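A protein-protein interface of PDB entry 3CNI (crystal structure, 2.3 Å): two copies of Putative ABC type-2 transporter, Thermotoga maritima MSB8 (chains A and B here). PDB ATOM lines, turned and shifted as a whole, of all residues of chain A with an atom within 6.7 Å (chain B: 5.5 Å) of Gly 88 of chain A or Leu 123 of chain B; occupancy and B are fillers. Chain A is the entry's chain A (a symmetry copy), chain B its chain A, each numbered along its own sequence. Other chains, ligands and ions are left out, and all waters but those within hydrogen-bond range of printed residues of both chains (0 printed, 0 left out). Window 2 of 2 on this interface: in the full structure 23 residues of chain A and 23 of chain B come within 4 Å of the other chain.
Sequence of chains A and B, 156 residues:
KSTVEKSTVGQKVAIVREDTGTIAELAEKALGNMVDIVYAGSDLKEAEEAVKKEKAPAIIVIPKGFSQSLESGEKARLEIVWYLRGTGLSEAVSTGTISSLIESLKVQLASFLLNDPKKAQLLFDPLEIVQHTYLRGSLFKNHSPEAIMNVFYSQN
The backbone NH (N) of Gly 88 of chain A sits at hydrogen-bond distance from the side-chain carboxylate (OE1) of Glu 91 of chain A, 3.1 Å away. The side-chain hydroxyl (OG1) of Thr 87 of chain A is in hydrogen-bond range of the side-chain hydroxyl (OH) of Tyr 153 of chain A (3.2 Å).
Among the printed residues, pairs that only touch across the chains: Leu 89 of chain A with Ala 110 of chain B, Leu 89 of chain A with Leu 114 of chain B, Ala 92 of chain A with Leu 123 of chain B, Tyr 153 of chain A with Gln 121 of chain B, Met 149 of chain A with Phe 124 of chain B, Ala 92 of chain A with Phe 124 of chain B, Glu 91 of chain A with Phe 124 of chain B, Tyr 153 of chain A with Ala 120 of chain B and Gly 88 of chain A with Leu 123 of chain B.
Gly 88 of chain A touches one residue of chain B. Printed residues of chain B within 4 Å of Met 149 of chain A: Phe 124 (3.6 Å). Of the printed residues of chain B, Tyr 153 of chain A touches Ala 120 and Gln 121. Leu 113 of chain B touches none of the printed residues of chain A. Of the printed residues of chain A, Leu 114 of chain B touches Leu 89. Printed residues of chain A within 4 Å of Gln 121 of chain B: Tyr 153. The nearest residue of chain B that does not touch Gly 88 of chain A is Phe 124 of chain B (4.3 Å).
Of the 10 printed residues of chain A, 6 touch a printed residue of chain B. Hydrophobic or aromatic side chains of chain A that line the printed part of chain B: Leu 89, Ala 92, Met 149 and Tyr 153. Of the 12 printed residues of chain B, 6 touch a printed residue of chain A. Printed residues of chain B that touch a printed residue of chain A: Ala 110, Leu 114, Ala 120, Gln 121, Leu 123 and Phe 124. Along chain B the printed residues that touch a printed residue of chain A span positions 110 to 124.
No position is printed for both chains.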
ATOM      1  N   GLY A  86       8.398 -28.579 -24.114  1.00  0.00           N
ATOM      2  CA  GLY A  86       7.263 -28.026 -24.809  1.00  0.00           C
ATOM      3  C   GLY A  86       7.237 -26.525 -24.629  1.00  0.00           C
ATOM      4  O   GLY A  86       7.786 -25.965 -23.662  1.00  0.00           O
ATOM      5  N   THR A  87       6.568 -25.892 -25.577  1.00  0.00           N
ATOM      6  CA  THR A  87       6.536 -24.452 -25.674  1.00  0.00           C
ATOM      7  C   THR A  87       5.106 -23.946 -25.682  1.00  0.00           C
ATOM      8  O   THR A  87       4.747 -23.077 -26.484  1.00  0.00           O
ATOM      9  CB  THR A  87       7.324 -23.972 -26.897  1.00  0.00           C
ATOM     10  OG1 THR A  87       6.600 -24.202 -28.110  1.00  0.00           O
ATOM     11  CG2 THR A  87       8.670 -24.699 -26.960  1.00  0.00           C
ATOM     12  N   GLY A  88       4.316 -24.466 -24.736  1.00  0.00           N
ATOM     13  CA  GLY A  88       2.895 -24.139 -24.640  1.00  0.00           C
ATOM     14  C   GLY A  88       2.365 -23.609 -23.343  1.00  0.00           C
ATOM     15  O   GLY A  88       3.076 -23.264 -22.414  1.00  0.00           O
ATOM     16  N   LEU A  89       1.058 -23.601 -23.284  1.00  0.00           N
ATOM     17  CA  LEU A  89       0.370 -22.925 -22.215  1.00  0.00           C
ATOM     18  C   LEU A  89       0.890 -23.310 -20.839  1.00  0.00           C
ATOM     19  O   LEU A  89       0.978 -22.462 -19.959  1.00  0.00           O
ATOM     20  CB  LEU A  89      -1.141 -23.155 -22.296  1.00  0.00           C
ATOM     21  CG  LEU A  89      -2.049 -22.329 -21.360  1.00  0.00           C
ATOM     22  CD1 LEU A  89      -1.648 -20.841 -21.247  1.00  0.00           C
ATOM     23  CD2 LEU A  89      -3.538 -22.458 -21.742  1.00  0.00           C
ATOM     24  N   SER A  90       1.232 -24.583 -20.663  1.00  0.00           N
ATOM     25  CA  SER A  90       1.464 -25.142 -19.319  1.00  0.00           C
ATOM     26  C   SER A  90       2.799 -24.640 -18.854  1.00  0.00           C
ATOM     27  O   SER A  90       2.982 -24.264 -17.720  1.00  0.00           O
ATOM     28  CB  SER A  90       1.441 -26.684 -19.303  1.00  0.00           C
ATOM     29  OG  SER A  90       0.219 -27.189 -19.831  1.00  0.00           O
ATOM     30  N   GLU A  91       3.701 -24.597 -19.805  1.00  0.00           N
ATOM     31  CA  GLU A  91       5.086 -24.157 -19.609  1.00  0.00           C
ATOM     32  C   GLU A  91       5.136 -22.647 -19.316  1.00  0.00           C
ATOM     33  O   GLU A  91       5.919 -22.230 -18.499  1.00  0.00           O
ATOM     34  CB  GLU A  91       5.973 -24.517 -20.836  1.00  0.00           C
ATOM     35  CG  GLU A  91       6.336 -26.043 -20.991  1.00  0.00           C
ATOM     36  CD  GLU A  91       5.185 -26.931 -21.510  1.00  0.00           C
ATOM     37  OE1 GLU A  91       4.459 -26.559 -22.480  1.00  0.00           O
ATOM     38  OE2 GLU A  91       5.015 -28.040 -20.945  1.00  0.00           O
ATOM     39  N   ALA A  92       4.275 -21.882 -20.009  1.00  0.00           N
ATOM     40  CA  ALA A  92       4.095 -20.426 -19.831  1.00  0.00           C
ATOM     41  C   ALA A  92       3.527 -20.169 -18.457  1.00  0.00           C
ATOM     42  O   ALA A  92       3.950 -19.253 -17.752  1.00  0.00           O
ATOM     43  CB  ALA A  92       3.211 -19.774 -20.934  1.00  0.00           C
ATOM     44  N   VAL A  93       2.631 -21.036 -18.028  1.00  0.00           N
ATOM     45  CA  VAL A  93       2.008 -20.892 -16.706  1.00  0.00           C
ATOM     46  C   VAL A  93       2.997 -21.156 -15.589  1.00  0.00           C
ATOM     47  O   VAL A  93       3.038 -20.415 -14.590  1.00  0.00           O
ATOM     48  CB  VAL A  93       0.771 -21.777 -16.566  1.00  0.00           C
ATOM     49  CG1 VAL A  93       0.345 -21.939 -15.085  1.00  0.00           C
ATOM     50  CG2 VAL A  93      -0.360 -21.184 -17.452  1.00  0.00           C
ATOM     51  N   MET A 149      12.747 -18.461 -25.984  1.00  0.00           N
ATOM     52  CA  MET A 149      11.543 -18.455 -26.802  1.00  0.00           C
ATOM     53  C   MET A 149      11.550 -17.263 -27.724  1.00  0.00           C
ATOM     54  O   MET A 149      11.102 -17.375 -28.811  1.00  0.00           O
ATOM     55  CB  MET A 149      10.287 -18.447 -25.905  1.00  0.00           C
ATOM     56  CG  MET A 149      10.110 -19.732 -25.083  1.00  0.00           C
ATOM     57  SD  MET A 149       9.664 -21.232 -26.323  1.00  0.00           S
ATOM     58  CE  MET A 149      11.006 -22.496 -25.612  1.00  0.00           C
ATOM     59  N   TYR A 153      11.395 -17.614 -31.893  1.00  0.00           N
ATOM     60  CA  TYR A 153      10.178 -17.066 -32.480  1.00  0.00           C
ATOM     61  C   TYR A 153      10.434 -15.698 -33.139  1.00  0.00           C
ATOM     62  O   TYR A 153       9.505 -15.055 -33.622  1.00  0.00           O
ATOM     63  CB  TYR A 153       9.032 -16.987 -31.465  1.00  0.00           C
ATOM     64  CG  TYR A 153       8.335 -18.315 -31.170  1.00  0.00           C
ATOM     65  CD1 TYR A 153       7.453 -18.884 -32.093  1.00  0.00           C
ATOM     66  CD2 TYR A 153       8.520 -18.969 -29.952  1.00  0.00           C
ATOM     67  CE1 TYR A 153       6.796 -20.095 -31.832  1.00  0.00           C
ATOM     68  CE2 TYR A 153       7.858 -20.196 -29.646  1.00  0.00           C
ATOM     69  CZ  TYR A 153       6.998 -20.752 -30.607  1.00  0.00           C
ATOM     70  OH  TYR A 153       6.325 -21.937 -30.369  1.00  0.00           O
ATOM     71  N   LYS B 106       0.424 -12.058 -16.385  1.00  0.00           N
ATOM     72  CA  LYS B 106       0.914 -12.580 -17.623  1.00  0.00           C
ATOM     73  C   LYS B 106       0.296 -13.942 -17.831  1.00  0.00           C
ATOM     74  O   LYS B 106      -0.081 -14.304 -18.960  1.00  0.00           O
ATOM     75  CB  LYS B 106       2.408 -12.758 -17.557  1.00  0.00           C
ATOM     76  CG  LYS B 106       3.217 -11.443 -17.436  1.00  0.00           C
ATOM     77  CD  LYS B 106       4.682 -11.806 -17.386  1.00  0.00           C
ATOM     78  CE  LYS B 106       5.532 -10.561 -17.181  1.00  0.00           C
ATOM     79  NZ  LYS B 106       6.879 -11.009 -16.770  1.00  0.00           N
ATOM     80  N   ALA B 110      -2.899 -15.689 -20.753  1.00  0.00           N
ATOM     81  CA  ALA B 110      -2.307 -16.676 -21.646  1.00  0.00           C
ATOM     82  C   ALA B 110      -3.265 -17.330 -22.615  1.00  0.00           C
ATOM     83  O   ALA B 110      -2.927 -17.526 -23.772  1.00  0.00           O
ATOM     84  CB  ALA B 110      -1.522 -17.723 -20.852  1.00  0.00           C
ATOM     85  N   LEU B 113      -3.848 -15.867 -25.856  1.00  0.00           N
ATOM     86  CA  LEU B 113      -2.736 -15.832 -26.776  1.00  0.00           C
ATOM     87  C   LEU B 113      -2.600 -17.138 -27.487  1.00  0.00           C
ATOM     88  O   LEU B 113      -1.650 -17.344 -28.241  1.00  0.00           O
ATOM     89  CB  LEU B 113      -1.457 -15.498 -26.032  1.00  0.00           C
ATOM     90  CG  LEU B 113      -1.479 -14.204 -25.216  1.00  0.00           C
ATOM     91  CD1 LEU B 113      -0.167 -14.059 -24.444  1.00  0.00           C
ATOM     92  CD2 LEU B 113      -1.775 -13.005 -26.132  1.00  0.00           C
ATOM     93  N   LEU B 114      -3.550 -18.033 -27.261  1.00  0.00           N
ATOM     94  CA  LEU B 114      -3.475 -19.382 -27.863  1.00  0.00           C
ATOM     95  C   LEU B 114      -3.987 -19.378 -29.291  1.00  0.00           C
ATOM     96  O   LEU B 114      -3.808 -20.344 -30.016  1.00  0.00           O
ATOM     97  CB  LEU B 114      -4.232 -20.429 -27.026  1.00  0.00           C
ATOM     98  CG  LEU B 114      -3.608 -20.764 -25.674  1.00  0.00           C
ATOM     99  CD1 LEU B 114      -4.585 -21.676 -24.879  1.00  0.00           C
ATOM    100  CD2 LEU B 114      -2.182 -21.375 -25.823  1.00  0.00           C
ATOM    101  N   LYS B 119       1.116 -15.140 -31.998  1.00  0.00           N
ATOM    102  CA  LYS B 119       0.988 -14.783 -30.582  1.00  0.00           C
ATOM    103  C   LYS B 119       1.779 -15.670 -29.646  1.00  0.00           C
ATOM    104  O   LYS B 119       1.729 -15.449 -28.446  1.00  0.00           O
ATOM    105  CB  LYS B 119      -0.483 -14.803 -30.145  1.00  0.00           C
ATOM    106  CG  LYS B 119      -1.391 -13.862 -30.898  1.00  0.00           C
ATOM    107  CD  LYS B 119      -2.792 -13.981 -30.321  1.00  0.00           C
ATOM    108  CE  LYS B 119      -3.884 -13.250 -31.062  1.00  0.00           C
ATOM    109  NZ  LYS B 119      -5.197 -13.592 -30.365  1.00  0.00           N
ATOM    110  N   ALA B 120       2.552 -16.596 -30.193  1.00  0.00           N
ATOM    111  CA  ALA B 120       3.013 -17.759 -29.433  1.00  0.00           C
ATOM    112  C   ALA B 120       4.189 -17.463 -28.549  1.00  0.00           C
ATOM    113  O   ALA B 120       4.365 -18.077 -27.481  1.00  0.00           O
ATOM    114  CB  ALA B 120       3.343 -18.897 -30.370  1.00  0.00           C
ATOM    115  N   GLN B 121       5.002 -16.497 -28.991  1.00  0.00           N
ATOM    116  CA  GLN B 121       6.138 -15.918 -28.188  1.00  0.00           C
ATOM    117  C   GLN B 121       5.596 -15.278 -26.932  1.00  0.00           C
ATOM    118  O   GLN B 121       6.148 -15.381 -25.783  1.00  0.00           O
ATOM    119  CB  GLN B 121       6.846 -14.797 -28.992  1.00  0.00           C
ATOM    120  CG  GLN B 121       6.415 -14.711 -30.501  1.00  0.00           C
ATOM    121  N   LEU B 122       4.505 -14.564 -27.227  1.00  0.00           N
ATOM    122  CA  LEU B 122       3.918 -13.706 -26.204  1.00  0.00           C
ATOM    123  C   LEU B 122       3.504 -14.512 -24.978  1.00  0.00           C
ATOM    124  O   LEU B 122       3.339 -14.009 -23.945  1.00  0.00           O
ATOM    125  CB  LEU B 122       2.713 -12.948 -26.768  1.00  0.00           C
ATOM    126  CG  LEU B 122       3.005 -11.946 -27.886  1.00  0.00           C
ATOM    127  CD1 LEU B 122       1.712 -11.369 -28.440  1.00  0.00           C
ATOM    128  CD2 LEU B 122       3.923 -10.838 -27.390  1.00  0.00           C
ATOM    129  N   LEU B 123       3.400 -15.807 -25.187  1.00  0.00           N
ATOM    130  CA  LEU B 123       3.001 -16.692 -24.136  1.00  0.00           C
ATOM    131  C   LEU B 123       3.898 -16.502 -22.957  1.00  0.00           C
ATOM    132  O   LEU B 123       3.431 -16.313 -21.862  1.00  0.00           O
ATOM    133  CB  LEU B 123       3.061 -18.131 -24.604  1.00  0.00           C
ATOM    134  CG  LEU B 123       1.768 -18.730 -25.113  1.00  0.00           C
ATOM    135  CD1 LEU B 123       1.933 -20.215 -25.350  1.00  0.00           C
ATOM    136  CD2 LEU B 123       0.684 -18.465 -24.134  1.00  0.00           C
ATOM    137  N   PHE B 124       5.193 -16.560 -23.198  1.00  0.00           N
ATOM    138  CA  PHE B 124       6.174 -16.459 -22.155  1.00  0.00           C
ATOM    139  C   PHE B 124       6.510 -15.035 -21.792  1.00  0.00           C
ATOM    140  O   PHE B 124       6.840 -14.758 -20.678  1.00  0.00           O
ATOM    141  CB  PHE B 124       7.432 -17.189 -22.549  1.00  0.00           C
ATOM    142  CG  PHE B 124       7.260 -18.645 -22.678  1.00  0.00           C
ATOM    143  CD1 PHE B 124       6.756 -19.195 -23.821  1.00  0.00           C
ATOM    144  CD2 PHE B 124       7.612 -19.475 -21.668  1.00  0.00           C
ATOM    145  CE1 PHE B 124       6.596 -20.550 -23.935  1.00  0.00           C
ATOM    146  CE2 PHE B 124       7.451 -20.823 -21.785  1.00  0.00           C
ATOM    147  CZ  PHE B 124       6.945 -21.357 -22.923  1.00  0.00           C
ATOM    148  N   ASP B 125       6.325 -14.134 -22.721  1.00  0.00           N
ATOM    149  CA  ASP B 125       6.752 -12.796 -22.527  1.00  0.00           C
ATOM    150  C   ASP B 125       5.870 -11.835 -23.254  1.00  0.00           C
ATOM    151  O   ASP B 125       6.214 -11.320 -24.270  1.00  0.00           O
ATOM    152  CB  ASP B 125       8.176 -12.654 -22.979  1.00  0.00           C
ATOM    153  CG  ASP B 125       8.833 -11.428 -22.443  1.00  0.00           C
ATOM    154  OD1 ASP B 125       8.376 -10.882 -21.432  1.00  0.00           O
ATOM    155  OD2 ASP B 125       9.821 -11.015 -23.040  1.00  0.00           O
ATOM    156  N   PRO B 126       4.728 -11.572 -22.674  1.00  0.00           N
ATOM    157  CA  PRO B 126       3.666 -10.879 -23.357  1.00  0.00           C
ATOM    158  C   PRO B 126       3.768  -9.402 -23.152  1.00  0.00           C
ATOM    159  O   PRO B 126       3.198  -8.676 -23.922  1.00  0.00           O
ATOM    160  CB  PRO B 126       2.445 -11.408 -22.653  1.00  0.00           C
ATOM    161  CG  PRO B 126       2.932 -11.820 -21.391  1.00  0.00           C
ATOM    162  CD  PRO B 126       4.181 -12.454 -21.655  1.00  0.00           C
